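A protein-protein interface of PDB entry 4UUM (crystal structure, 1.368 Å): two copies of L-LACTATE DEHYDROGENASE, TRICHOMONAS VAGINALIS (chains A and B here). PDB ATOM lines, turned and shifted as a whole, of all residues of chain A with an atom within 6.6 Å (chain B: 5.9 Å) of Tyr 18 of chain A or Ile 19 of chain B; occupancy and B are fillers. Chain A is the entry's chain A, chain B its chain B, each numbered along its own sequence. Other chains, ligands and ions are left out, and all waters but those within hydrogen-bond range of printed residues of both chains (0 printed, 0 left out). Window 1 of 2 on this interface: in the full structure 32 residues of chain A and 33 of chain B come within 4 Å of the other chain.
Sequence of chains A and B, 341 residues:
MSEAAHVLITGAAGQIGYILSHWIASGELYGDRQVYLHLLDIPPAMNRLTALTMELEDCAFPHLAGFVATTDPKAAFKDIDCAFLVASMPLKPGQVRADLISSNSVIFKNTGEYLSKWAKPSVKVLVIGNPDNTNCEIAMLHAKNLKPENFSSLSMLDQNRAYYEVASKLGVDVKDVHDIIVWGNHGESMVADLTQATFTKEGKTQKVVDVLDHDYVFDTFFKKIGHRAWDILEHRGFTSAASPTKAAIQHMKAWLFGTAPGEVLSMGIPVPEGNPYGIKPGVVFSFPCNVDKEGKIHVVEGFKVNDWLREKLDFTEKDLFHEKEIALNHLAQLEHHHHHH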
ATOM      1  N   ILE A   9     -31.159  19.074 -21.448  1.00  0.00           N
ATOM      2  CA  ILE A   9     -30.222  19.663 -22.386  1.00  0.00           C
ATOM      3  C   ILE A   9     -30.336  18.891 -23.692  1.00  0.00           C
ATOM      4  O   ILE A   9     -30.098  17.681 -23.708  1.00  0.00           O
ATOM      5  CB  ILE A   9     -28.762  19.560 -21.881  1.00  0.00           C
ATOM      6  CG1 ILE A   9     -28.638  20.247 -20.522  1.00  0.00           C
ATOM      7  CG2 ILE A   9     -27.792  20.193 -22.881  1.00  0.00           C
ATOM      8  CD1 ILE A   9     -27.295  19.970 -19.830  1.00  0.00           C
ATOM      9  N   GLY A  11     -29.051  18.366 -27.774  1.00  0.00           N
ATOM     10  CA  GLY A  11     -27.720  18.377 -28.333  1.00  0.00           C
ATOM     11  C   GLY A  11     -26.657  18.093 -27.278  1.00  0.00           C
ATOM     12  O   GLY A  11     -25.555  18.622 -27.327  1.00  0.00           O
ATOM     13  N   ALA A  12     -26.992  17.236 -26.323  1.00  0.00           N
ATOM     14  CA  ALA A  12     -26.176  17.071 -25.122  1.00  0.00           C
ATOM     15  C   ALA A  12     -24.775  16.563 -25.369  1.00  0.00           C
ATOM     16  O   ALA A  12     -23.882  16.811 -24.556  1.00  0.00           O
ATOM     17  CB  ALA A  12     -26.881  16.170 -24.122  1.00  0.00           C
ATOM     18  N   ALA A  13     -24.580  15.847 -26.464  1.00  0.00           N
ATOM     19  CA  ALA A  13     -23.267  15.294 -26.779  1.00  0.00           C
ATOM     20  C   ALA A  13     -22.320  16.306 -27.412  1.00  0.00           C
ATOM     21  O   ALA A  13     -21.144  16.007 -27.615  1.00  0.00           O
ATOM     22  CB  ALA A  13     -23.417  14.081 -27.671  1.00  0.00           C
ATOM     23  N   GLY A  14     -22.818  17.497 -27.722  1.00  0.00           N
ATOM     24  CA  GLY A  14     -22.001  18.497 -28.371  1.00  0.00           C
ATOM     25  C   GLY A  14     -21.135  19.254 -27.375  1.00  0.00           C
ATOM     26  O   GLY A  14     -21.162  18.989 -26.176  1.00  0.00           O
ATOM     27  N   GLN A  15     -20.379  20.209 -27.876  1.00  0.00           N
ATOM     28  CA  GLN A  15     -19.431  20.949 -27.048  1.00  0.00           C
ATOM     29  C   GLN A  15     -20.111  21.768 -25.941  1.00  0.00           C
ATOM     30  O   GLN A  15     -19.645  21.795 -24.807  1.00  0.00           O
ATOM     31  CB  GLN A  15     -18.605  21.900 -27.913  1.00  0.00           C
ATOM     32  CG  GLN A  15     -17.660  21.260 -28.898  1.00  0.00           C
ATOM     33  CD  GLN A  15     -16.744  22.296 -29.535  1.00  0.00           C
ATOM     34  OE1 GLN A  15     -17.170  23.416 -29.855  1.00  0.00           O
ATOM     35  NE2 GLN A  15     -15.476  21.939 -29.696  1.00  0.00           N
ATOM     36  N   ILE A  16     -21.197  22.449 -26.268  1.00  0.00           N
ATOM     37  CA  ILE A  16     -21.944  23.184 -25.268  1.00  0.00           C
ATOM     38  C   ILE A  16     -22.534  22.203 -24.260  1.00  0.00           C
ATOM     39  O   ILE A  16     -22.409  22.416 -23.062  1.00  0.00           O
ATOM     40  CB  ILE A  16     -23.030  24.065 -25.906  1.00  0.00           C
ATOM     41  CG1 ILE A  16     -22.373  25.245 -26.644  1.00  0.00           C
ATOM     42  CG2 ILE A  16     -24.000  24.585 -24.850  1.00  0.00           C
ATOM     43  CD1 ILE A  16     -23.313  26.055 -27.531  1.00  0.00           C
ATOM     44  N   GLY A  17     -23.193  21.147 -24.737  1.00  0.00           N
ATOM     45  CA  GLY A  17     -23.789  20.164 -23.846  1.00  0.00           C
ATOM     46  C   GLY A  17     -22.796  19.597 -22.834  1.00  0.00           C
ATOM     47  O   GLY A  17     -23.121  19.389 -21.658  1.00  0.00           O
ATOM     48  N   TYR A  18     -21.596  19.330 -23.314  1.00  0.00           N
ATOM     49  CA  TYR A  18     -20.531  18.754 -22.511  1.00  0.00           C
ATOM     50  C   TYR A  18     -20.227  19.647 -21.308  1.00  0.00           C
ATOM     51  O   TYR A  18     -20.165  19.190 -20.174  1.00  0.00           O
ATOM     52  CB  TYR A  18     -19.294  18.617 -23.387  1.00  0.00           C
ATOM     53  CG  TYR A  18     -18.084  17.990 -22.741  1.00  0.00           C
ATOM     54  CD1 TYR A  18     -18.020  16.627 -22.484  1.00  0.00           C
ATOM     55  CD2 TYR A  18     -16.983  18.761 -22.417  1.00  0.00           C
ATOM     56  CE1 TYR A  18     -16.874  16.047 -21.933  1.00  0.00           C
ATOM     57  CE2 TYR A  18     -15.844  18.199 -21.862  1.00  0.00           C
ATOM     58  CZ  TYR A  18     -15.809  16.848 -21.615  1.00  0.00           C
ATOM     59  OH  TYR A  18     -14.670  16.300 -21.082  1.00  0.00           O
ATOM     60  N   ILE A  19     -19.991  20.932 -21.580  1.00  0.00           N
ATOM     61  CA  ILE A  19     -19.626  21.875 -20.525  1.00  0.00           C
ATOM     62  C   ILE A  19     -20.841  22.216 -19.653  1.00  0.00           C
ATOM     63  O   ILE A  19     -20.746  22.275 -18.423  1.00  0.00           O
ATOM     64  CB  ILE A  19     -18.996  23.130 -21.123  1.00  0.00           C
ATOM     65  CG1 ILE A  19     -17.762  22.752 -21.937  1.00  0.00           C
ATOM     66  CG2 ILE A  19     -18.639  24.123 -20.036  1.00  0.00           C
ATOM     67  CD1 ILE A  19     -17.189  23.899 -22.730  1.00  0.00           C
ATOM     68  N   LEU A  20     -21.974  22.476 -20.314  1.00  0.00           N
ATOM     69  CA  LEU A  20     -23.204  22.860 -19.632  1.00  0.00           C
ATOM     70  C   LEU A  20     -23.639  21.780 -18.612  1.00  0.00           C
ATOM     71  O   LEU A  20     -23.994  22.085 -17.470  1.00  0.00           O
ATOM     72  CB  LEU A  20     -24.281  23.159 -20.686  1.00  0.00           C
ATOM     73  CG  LEU A  20     -25.651  23.599 -20.194  1.00  0.00           C
ATOM     74  CD1 LEU A  20     -25.594  24.908 -19.413  1.00  0.00           C
ATOM     75  CD2 LEU A  20     -26.598  23.748 -21.369  1.00  0.00           C
ATOM     76  N   SER A  21     -23.594  20.518 -19.031  1.00  0.00           N
ATOM     77  CA  SER A  21     -24.018  19.437 -18.144  1.00  0.00           C
ATOM     78  C   SER A  21     -23.132  19.369 -16.890  1.00  0.00           C
ATOM     79  O   SER A  21     -23.653  19.246 -15.774  1.00  0.00           O
ATOM     80  CB  SER A  21     -24.034  18.093 -18.877  1.00  0.00           C
ATOM     81  OG  SER A  21     -22.733  17.747 -19.307  1.00  0.00           O
ATOM     82  N   HIS A  22     -21.819  19.482 -17.052  1.00  0.00           N
ATOM     83  CA  HIS A  22     -20.919  19.444 -15.912  1.00  0.00           C
ATOM     84  C   HIS A  22     -21.121  20.661 -14.984  1.00  0.00           C
ATOM     85  O   HIS A  22     -21.150  20.519 -13.771  1.00  0.00           O
ATOM     86  CB  HIS A  22     -19.471  19.371 -16.387  1.00  0.00           C
ATOM     87  CG  HIS A  22     -19.038  17.994 -16.780  1.00  0.00           C
ATOM     88  ND1 HIS A  22     -19.197  17.498 -18.060  1.00  0.00           N
ATOM     89  CD2 HIS A  22     -18.395  17.029 -16.076  1.00  0.00           C
ATOM     90  CE1 HIS A  22     -18.712  16.269 -18.110  1.00  0.00           C
ATOM     91  NE2 HIS A  22     -18.227  15.960 -16.921  1.00  0.00           N
ATOM     92  N   TRP A  23     -21.292  21.838 -15.587  1.00  0.00           N
ATOM     93  CA  TRP A  23     -21.414  23.076 -14.819  1.00  0.00           C
ATOM     94  C   TRP A  23     -22.692  22.994 -13.970  1.00  0.00           C
ATOM     95  O   TRP A  23     -22.698  23.298 -12.778  1.00  0.00           O
ATOM     96  CB  TRP A  23     -21.434  24.276 -15.774  1.00  0.00           C
ATOM     97  CG  TRP A  23     -20.957  25.594 -15.198  1.00  0.00           C
ATOM     98  CD1 TRP A  23     -21.035  25.994 -13.902  1.00  0.00           C
ATOM     99  CD2 TRP A  23     -20.346  26.687 -15.917  1.00  0.00           C
ATOM    100  NE1 TRP A  23     -20.522  27.262 -13.760  1.00  0.00           N
ATOM    101  CE2 TRP A  23     -20.081  27.701 -14.980  1.00  0.00           C
ATOM    102  CE3 TRP A  23     -19.991  26.896 -17.249  1.00  0.00           C
ATOM    103  CZ2 TRP A  23     -19.493  28.921 -15.335  1.00  0.00           C
ATOM    104  CZ3 TRP A  23     -19.388  28.106 -17.599  1.00  0.00           C
ATOM    105  CH2 TRP A  23     -19.154  29.101 -16.644  1.00  0.00           C
ATOM    106  N   ARG A  48     -20.784   9.454 -28.149  1.00  0.00           N
ATOM    107  CA  ARG A  48     -20.319  10.677 -27.497  1.00  0.00           C
ATOM    108  C   ARG A  48     -21.178  10.976 -26.282  1.00  0.00           C
ATOM    109  O   ARG A  48     -20.699  11.521 -25.297  1.00  0.00           O
ATOM    110  CB  ARG A  48     -20.344  11.878 -28.444  1.00  0.00           C
ATOM    111  CG  ARG A  48     -19.139  11.975 -29.358  1.00  0.00           C
ATOM    112  CD  ARG A  48     -18.753  13.427 -29.633  1.00  0.00           C
ATOM    113  NE  ARG A  48     -19.914  14.295 -29.835  1.00  0.00           N
ATOM    114  CZ  ARG A  48     -20.702  14.270 -30.907  1.00  0.00           C
ATOM    115  NH1 ARG A  48     -20.476  13.405 -31.888  1.00  0.00           N
ATOM    116  NH2 ARG A  48     -21.730  15.105 -30.991  1.00  0.00           N
ATOM    117  N   ALA A  51     -19.977   8.729 -23.560  1.00  0.00           N
ATOM    118  CA  ALA A  51     -18.732   9.295 -23.035  1.00  0.00           C
ATOM    119  C   ALA A  51     -19.018  10.433 -22.064  1.00  0.00           C
ATOM    120  O   ALA A  51     -18.380  10.537 -21.013  1.00  0.00           O
ATOM    121  CB  ALA A  51     -17.855   9.781 -24.169  1.00  0.00           C
ATOM    122  N   LEU A  52     -19.966  11.298 -22.427  1.00  0.00           N
ATOM    123  CA  LEU A  52     -20.359  12.372 -21.518  1.00  0.00           C
ATOM    124  C   LEU A  52     -20.837  11.803 -20.180  1.00  0.00           C
ATOM    125  O   LEU A  52     -20.408  12.269 -19.112  1.00  0.00           O
ATOM    126  CB  LEU A  52     -21.437  13.263 -22.153  1.00  0.00           C
ATOM    127  CG  LEU A  52     -22.095  14.257 -21.189  1.00  0.00           C
ATOM    128  CD1 LEU A  52     -21.068  15.191 -20.549  1.00  0.00           C
ATOM    129  CD2 LEU A  52     -23.171  15.065 -21.892  1.00  0.00           C
ATOM    130  N   GLU A  55     -17.945  10.685 -17.893  1.00  0.00           N
ATOM    131  CA  GLU A  55     -17.219  11.748 -17.204  1.00  0.00           C
ATOM    132  C   GLU A  55     -18.052  12.384 -16.106  1.00  0.00           C
ATOM    133  O   GLU A  55     -17.520  12.736 -15.067  1.00  0.00           O
ATOM    134  CB  GLU A  55     -16.678  12.808 -18.164  1.00  0.00           C
ATOM    135  CG  GLU A  55     -15.428  12.353 -18.913  1.00  0.00           C
ATOM    136  CD  GLU A  55     -14.646  13.508 -19.472  1.00  0.00           C
ATOM    137  OE1 GLU A  55     -13.944  14.192 -18.695  1.00  0.00           O
ATOM    138  OE2 GLU A  55     -14.755  13.756 -20.692  1.00  0.00           O
ATOM    139  N   LEU A  56     -19.358  12.541 -16.328  1.00  0.00           N
ATOM    140  CA  LEU A  56     -20.227  13.043 -15.264  1.00  0.00           C
ATOM    141  C   LEU A  56     -20.122  12.130 -14.045  1.00  0.00           C
ATOM    142  O   LEU A  56     -19.985  12.610 -12.926  1.00  0.00           O
ATOM    143  CB  LEU A  56     -21.686  13.153 -15.710  1.00  0.00           C
ATOM    144  CG  LEU A  56     -22.002  14.247 -16.735  1.00  0.00           C
ATOM    145  CD1 LEU A  56     -23.405  14.044 -17.281  1.00  0.00           C
ATOM    146  CD2 LEU A  56     -21.848  15.616 -16.107  1.00  0.00           C
ATOM    147  N   ALA A 242     -17.744  27.536 -24.344  1.00  0.00           N
ATOM    148  CA  ALA A 242     -17.711  27.975 -22.955  1.00  0.00           C
ATOM    149  C   ALA A 242     -18.466  29.292 -22.726  1.00  0.00           C
ATOM    150  O   ALA A 242     -19.195  29.441 -21.735  1.00  0.00           O
ATOM    151  CB  ALA A 242     -16.268  28.101 -22.469  1.00  0.00           C
ATOM    152  N   GLY B  14      -5.271  23.600 -24.506  1.00  0.00           N
ATOM    153  CA  GLY B  14      -5.925  22.311 -24.610  1.00  0.00           C
ATOM    154  C   GLY B  14      -7.301  22.309 -23.979  1.00  0.00           C
ATOM    155  O   GLY B  14      -7.756  23.317 -23.427  1.00  0.00           O
ATOM    156  N   GLN B  15      -7.979  21.174 -24.043  1.00  0.00           N
ATOM    157  CA  GLN B  15      -9.346  21.114 -23.539  1.00  0.00           C
ATOM    158  C   GLN B  15      -9.426  21.321 -22.029  1.00  0.00           C
ATOM    159  O   GLN B  15     -10.348  21.960 -21.543  1.00  0.00           O
ATOM    160  CB  GLN B  15     -10.006  19.796 -23.908  1.00  0.00           C
ATOM    161  CG  GLN B  15     -11.506  19.788 -23.673  1.00  0.00           C
ATOM    162  CD  GLN B  15     -12.199  21.020 -24.227  1.00  0.00           C
ATOM    163  OE1 GLN B  15     -12.819  21.770 -23.482  1.00  0.00           O
ATOM    164  NE2 GLN B  15     -12.096  21.231 -25.539  1.00  0.00           N
ATOM    165  N   ILE B  16      -8.481  20.761 -21.280  1.00  0.00           N
ATOM    166  CA  ILE B  16      -8.482  20.999 -19.838  1.00  0.00           C
ATOM    167  C   ILE B  16      -8.300  22.509 -19.564  1.00  0.00           C
ATOM    168  O   ILE B  16      -9.041  23.106 -18.794  1.00  0.00           O
ATOM    169  CB  ILE B  16      -7.416  20.138 -19.121  1.00  0.00           C
ATOM    170  CG1 ILE B  16      -7.866  18.683 -19.146  1.00  0.00           C
ATOM    171  CG2 ILE B  16      -7.211  20.639 -17.710  1.00  0.00           C
ATOM    172  CD1 ILE B  16      -6.801  17.667 -18.657  1.00  0.00           C
ATOM    173  N   GLY B  17      -7.316  23.124 -20.195  1.00  0.00           N
ATOM    174  CA  GLY B  17      -7.073  24.540 -19.989  1.00  0.00           C
ATOM    175  C   GLY B  17      -8.282  25.393 -20.318  1.00  0.00           C
ATOM    176  O   GLY B  17      -8.572  26.379 -19.631  1.00  0.00           O
ATOM    177  N   TYR B  18      -8.997  24.995 -21.365  1.00  0.00           N
ATOM    178  CA  TYR B  18     -10.186  25.711 -21.825  1.00  0.00           C
ATOM    179  C   TYR B  18     -11.255  25.727 -20.743  1.00  0.00           C
ATOM    180  O   TYR B  18     -11.801  26.783 -20.393  1.00  0.00           O
ATOM    181  CB  TYR B  18     -10.697  25.027 -23.090  1.00  0.00           C
ATOM    182  CG  TYR B  18     -11.908  25.641 -23.753  1.00  0.00           C
ATOM    183  CD1 TYR B  18     -11.805  26.816 -24.490  1.00  0.00           C
ATOM    184  CD2 TYR B  18     -13.138  25.009 -23.688  1.00  0.00           C
ATOM    185  CE1 TYR B  18     -12.924  27.359 -25.132  1.00  0.00           C
ATOM    186  CE2 TYR B  18     -14.243  25.525 -24.325  1.00  0.00           C
ATOM    187  CZ  TYR B  18     -14.131  26.694 -25.043  1.00  0.00           C
ATOM    188  OH  TYR B  18     -15.238  27.194 -25.675  1.00  0.00           O
ATOM    189  N   ILE B  19     -11.550  24.557 -20.193  1.00  0.00           N
ATOM    190  CA  ILE B  19     -12.591  24.464 -19.174  1.00  0.00           C
ATOM    191  C   ILE B  19     -12.098  25.036 -17.847  1.00  0.00           C
ATOM    192  O   ILE B  19     -12.827  25.774 -17.179  1.00  0.00           O
ATOM    193  CB  ILE B  19     -13.089  23.008 -19.010  1.00  0.00           C
ATOM    194  CG1 ILE B  19     -13.620  22.479 -20.338  1.00  0.00           C
ATOM    195  CG2 ILE B  19     -14.117  22.921 -17.902  1.00  0.00           C
ATOM    196  CD1 ILE B  19     -13.914  21.012 -20.350  1.00  0.00           C
ATOM    197  N   LEU B  20     -10.887  24.660 -17.446  1.00  0.00           N
ATOM    198  CA  LEU B  20     -10.301  25.108 -16.199  1.00  0.00           C
ATOM    199  C   LEU B  20     -10.244  26.629 -16.118  1.00  0.00           C
ATOM    200  O   LEU B  20     -10.572  27.217 -15.090  1.00  0.00           O
ATOM    201  CB  LEU B  20      -8.902  24.506 -16.047  1.00  0.00           C
ATOM    202  CG  LEU B  20      -8.153  24.739 -14.746  1.00  0.00           C
ATOM    203  CD1 LEU B  20      -8.914  24.196 -13.520  1.00  0.00           C
ATOM    204  CD2 LEU B  20      -6.782  24.086 -14.905  1.00  0.00           C
ATOM    205  N   SER B  21      -9.792  27.282 -17.180  1.00  0.00           N
ATOM    206  CA  SER B  21      -9.693  28.738 -17.161  1.00  0.00           C
ATOM    207  C   SER B  21     -11.062  29.383 -16.951  1.00  0.00           C
ATOM    208  O   SER B  21     -11.180  30.289 -16.140  1.00  0.00           O
ATOM    209  CB  SER B  21      -9.016  29.278 -18.430  1.00  0.00           C
ATOM    210  OG  SER B  21      -9.735  28.944 -19.600  1.00  0.00           O
ATOM    211  N   HIS B  22     -12.088  28.901 -17.638  1.00  0.00           N
ATOM    212  CA  HIS B  22     -13.412  29.474 -17.475  1.00  0.00           C
ATOM    213  C   HIS B  22     -13.980  29.212 -16.076  1.00  0.00           C
ATOM    214  O   HIS B  22     -14.565  30.093 -15.467  1.00  0.00           O
ATOM    215  CB  HIS B  22     -14.380  28.959 -18.540  1.00  0.00           C
ATOM    216  CG  HIS B  22     -14.224  29.619 -19.872  1.00  0.00           C
ATOM    217  ND1 HIS B  22     -13.291  29.219 -20.805  1.00  0.00           N
ATOM    218  CD2 HIS B  22     -14.888  30.668 -20.424  1.00  0.00           C
ATOM    219  CE1 HIS B  22     -13.381  30.003 -21.867  1.00  0.00           C
ATOM    220  NE2 HIS B  22     -14.343  30.885 -21.664  1.00  0.00           N
ATOM    221  N   TRP B  23     -13.761  28.013 -15.565  1.00  0.00           N
ATOM    222  CA  TRP B  23     -14.286  27.641 -14.261  1.00  0.00           C
ATOM    223  C   TRP B  23     -13.667  28.533 -13.204  1.00  0.00           C
ATOM    224  O   TRP B  23     -14.363  29.081 -12.348  1.00  0.00           O
ATOM    225  CB  TRP B  23     -13.984  26.170 -13.972  1.00  0.00           C
ATOM    226  CG  TRP B  23     -14.975  25.469 -13.081  1.00  0.00           C
ATOM    227  CD1 TRP B  23     -15.750  26.029 -12.111  1.00  0.00           C
ATOM    228  CD2 TRP B  23     -15.283  24.073 -13.085  1.00  0.00           C
ATOM    229  NE1 TRP B  23     -16.511  25.061 -11.493  1.00  0.00           N
ATOM    230  CE2 TRP B  23     -16.252  23.852 -12.082  1.00  0.00           C
ATOM    231  CE3 TRP B  23     -14.835  22.985 -13.841  1.00  0.00           C
ATOM    232  CZ2 TRP B  23     -16.783  22.593 -11.821  1.00  0.00           C
ATOM    233  CZ3 TRP B  23     -15.369  21.736 -13.579  1.00  0.00           C
ATOM    234  CH2 TRP B  23     -16.324  21.549 -12.575  1.00  0.00           C
ATOM    235  N   ILE B  24     -12.350  28.679 -13.258  1.00  0.00           N
ATOM    236  CA  ILE B  24     -11.661  29.547 -12.319  1.00  0.00           C
ATOM    237  C   ILE B  24     -12.116  31.009 -12.456  1.00  0.00           C
ATOM    238  O   ILE B  24     -12.371  31.673 -11.449  1.00  0.00           O
ATOM    239  CB  ILE B  24     -10.131  29.439 -12.462  1.00  0.00           C
ATOM    240  CG1 ILE B  24      -9.669  28.041 -12.030  1.00  0.00           C
ATOM    241  CG2 ILE B  24      -9.425  30.478 -11.620  1.00  0.00           C
ATOM    242  CD1 ILE B  24      -8.239  27.731 -12.349  1.00  0.00           C
ATOM    243  N   ARG B 236     -15.076   8.818 -26.432  1.00  0.00           N
ATOM    244  CA  ARG B 236     -14.967  10.263 -26.670  1.00  0.00           C
ATOM    245  C   ARG B 236     -14.102  10.629 -27.879  1.00  0.00           C
ATOM    246  O   ARG B 236     -14.269  11.703 -28.461  1.00  0.00           O
ATOM    247  CB  ARG B 236     -14.402  10.946 -25.411  1.00  0.00           C
ATOM    248  CG  ARG B 236     -14.143  12.458 -25.494  1.00  0.00           C
ATOM    249  CD  ARG B 236     -13.764  13.016 -24.121  1.00  0.00           C
ATOM    250  NE  ARG B 236     -13.079  14.311 -24.174  1.00  0.00           N
ATOM    251  CZ  ARG B 236     -13.679  15.479 -24.392  1.00  0.00           C
ATOM    252  NH1 ARG B 236     -14.985  15.535 -24.606  1.00  0.00           N
ATOM    253  NH2 ARG B 236     -12.962  16.596 -24.410  1.00  0.00           N
ATOM    254  N   THR B 239      -9.030  12.204 -24.785  1.00  0.00           N
ATOM    255  CA  THR B 239      -8.922  11.936 -23.353  1.00  0.00           C
ATOM    256  C   THR B 239      -9.924  12.775 -22.568  1.00  0.00           C
ATOM    257  O   THR B 239     -10.451  13.767 -23.076  1.00  0.00           O
ATOM    258  CB  THR B 239      -7.503  12.216 -22.827  1.00  0.00           C
ATOM    259  OG1 THR B 239      -7.120  13.560 -23.134  1.00  0.00           O
ATOM    260  CG2 THR B 239      -6.511  11.263 -23.458  1.00  0.00           C
ATOM    261  N   SER B 240     -10.177  12.356 -21.335  1.00  0.00           N
ATOM    262  CA  SER B 240     -11.021  13.076 -20.386  1.00  0.00           C
ATOM    263  C   SER B 240     -10.578  14.525 -20.274  1.00  0.00           C
ATOM    264  O   SER B 240      -9.369  14.816 -20.405  1.00  0.00           O
ATOM    265  CB  SER B 240     -10.920  12.413 -19.002  1.00  0.00           C
ATOM    266  OG  SER B 240      -9.626  12.587 -18.415  1.00  0.00           O
ATOM    267  N   ALA B 241     -11.521  15.425 -20.013  1.00  0.00           N
ATOM    268  CA  ALA B 241     -11.183  16.831 -19.818  1.00  0.00           C
ATOM    269  C   ALA B 241     -12.008  17.460 -18.693  1.00  0.00           C
ATOM    270  O   ALA B 241     -11.456  18.008 -17.749  1.00  0.00           O
ATOM    271  CB  ALA B 241     -11.335  17.589 -21.106  1.00  0.00           C
ATOM    272  N   ALA B 242     -13.330  17.400 -18.793  1.00  0.00           N
ATOM    273  CA  ALA B 242     -14.162  17.972 -17.737  1.00  0.00           C
ATOM    274  C   ALA B 242     -13.940  17.293 -16.388  1.00  0.00           C
ATOM    275  O   ALA B 242     -13.885  17.964 -15.351  1.00  0.00           O
ATOM    276  CB  ALA B 242     -15.625  17.928 -18.127  1.00  0.00           C
ATOM    277  N   SER B 243     -13.779  15.971 -16.378  1.00  0.00           N
ATOM    278  CA  SER B 243     -13.608  15.267 -15.102  1.00  0.00           C
ATOM    279  C   SER B 243     -12.252  15.491 -14.401  1.00  0.00           C
ATOM    280  O   SER B 243     -12.220  15.728 -13.195  1.00  0.00           O
ATOM    281  CB  SER B 243     -13.990  13.788 -15.202  1.00  0.00           C
ATOM    282  OG  SER B 243     -13.255  13.098 -16.184  1.00  0.00           O
ATOM    283  N   THR B 245     -10.599  18.193 -14.807  1.00  0.00           N
ATOM    284  CA  THR B 245     -10.692  19.596 -14.430  1.00  0.00           C
ATOM    285  C   THR B 245     -11.436  19.751 -13.112  1.00  0.00           C
ATOM    286  O   THR B 245     -10.999  20.478 -12.227  1.00  0.00           O
ATOM    287  CB  THR B 245     -11.372  20.443 -15.530  1.00  0.00           C
ATOM    288  OG1 THR B 245     -10.590  20.418 -16.730  1.00  0.00           O
ATOM    289  CG2 THR B 245     -11.526  21.894 -15.066  1.00  0.00           C
ATOM    290  N   ILE B 249      -9.674  21.439  -9.730  1.00  0.00           N
ATOM    291  CA  ILE B 249     -10.215  22.575  -8.992  1.00  0.00           C
ATOM    292  C   ILE B 249     -10.499  22.144  -7.568  1.00  0.00           C
ATOM    293  O   ILE B 249     -10.182  22.851  -6.623  1.00  0.00           O
ATOM    294  CB  ILE B 249     -11.465  23.141  -9.681  1.00  0.00           C
ATOM    295  CG1 ILE B 249     -11.020  23.850 -10.960  1.00  0.00           C
ATOM    296  CG2 ILE B 249     -12.206  24.128  -8.785  1.00  0.00           C
ATOM    297  CD1 ILE B 249     -12.132  24.253 -11.844  1.00  0.00           C
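The side-chain hydroxyl (OH) of Tyr 18 of chain A is in hydrogen-bond range of the backbone NH (N) of Ala 241 of chain B (3.4 Å). OH of Tyr 18 of chain A is in hydrogen-bond range of N of Ala 242 of chain B, 2.9 Å away. The guanidinium group (NE) of Arg 236 of chain B is in salt-bridge range of the side-chain carboxylate (OE2) of Glu 55 of chain A (3.9 Å). The backbone NH (N) of Ala 241 of chain B lies within hydrogen-bond range of the side-chain carboxylate (OE1) of Glu 55 of chain A. N of Ala 242 of chain B lies within hydrogen-bond range of OE1 of Glu 55 of chain A, at 3.3 Å. OG of Ser 243 of chain B lies within hydrogen-bond range of OE1 of Glu 55 of chain A, at 2.8 Å. N of Ala 242 of chain A sits at hydrogen-bond distance from OH of Tyr 18 of chain B (2.9 Å).
The backbone carbonyl oxygen (O) of Tyr 18 of chain A lies within hydrogen-bond range of the side-chain hydroxyl (OG) of Ser 21 of chain A (3.1 Å). O of Tyr 18 of chain A lies within hydrogen-bond range of ND1 of His 22 of chain A (2.9 Å). OE2 of Glu 55 of chain A sits at hydrogen-bond distance from OH of Tyr 18 of chain A (2.6 Å). ND1 of His 22 of chain B is in hydrogen-bond range of O of Tyr 18 of chain B, 2.9 Å away.
Tyr 18 of chain A touches Ile 19 of chain B. Tyr 18 of chain A touches Arg 236 of chain B. CD1 of Ile 19 of chain A touches CE2 of Tyr 18 of chain B, at 3.7 Å. Ala 242 of chain B touches His 22 of chain A. N of Arg 236 of chain B touches CB of Ala 51 of chain A, at 3.7 Å. OE1 of Glu 55 of chain A touches CB of Ser 240 of chain B, 3.5 Å away. CB of Ala 242 of chain A touches NE2 of His 22 of chain B, 3.5 Å away.
Ile 19 of chain B touches one residue of chain A. Of the printed residues of chain B, Ile 19 of chain A touches Tyr 18. Printed residues of chain B within 4 Å of Ala 242 of chain A: Tyr 18 (2.9 Å) and His 22 (3.5 Å). Printed residues of chain A within 4 Å of His 22 of chain B: Ala 242 (3.5 Å). Of the printed residues of chain A, Ala 241 of chain B touches Tyr 18 (3.4 Å) and Glu 55 (3.0 Å). Of the printed residues of chain A, Arg 236 of chain B touches Tyr 18, Ala 51 and Glu 55.
Of the 19 printed residues of chain B, 8 touch a printed residue of chain A. Printed residues of chain B that touch a printed residue of chain A: Tyr 18, Ile 19, His 22, Arg 236, Ser 240, Ala 241, Ala 242 and Ser 243. Hydrophobic or aromatic side chains of chain B within 4 Å of the printed part of chain A: Tyr 18, Ile 19, His 22, Ala 241 and Ala 242. Hydrophobic or aromatic side chains of chain A that line the printed part of chain B: Tyr 18, Ile 19, His 22, Ala 51 and Ala 242. Among the printed residues, Asp or Glu carboxylates within 4 Å of a Lys or Arg side-chain nitrogen of the other chain: Glu 55 of chain A with Arg 236 of chain B.
Tyr 18 of chain A touches Ile 19 of chain B, and with the chains exchanged Ile 19 of chain A touches Tyr 18 of chain B. His 22 of chain A touches Ala 242 of chain B, and with the chains exchanged Ala 242 of chain A touches His 22 of chain B. Positions printed for both chains: 14, 15, 16, 17, 18, 19, 20, 21, 22, 23 and 242. Of the 14 pairs that touch across the chains among the printed residues, 6 have their exchanged pair printed and touching as well.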
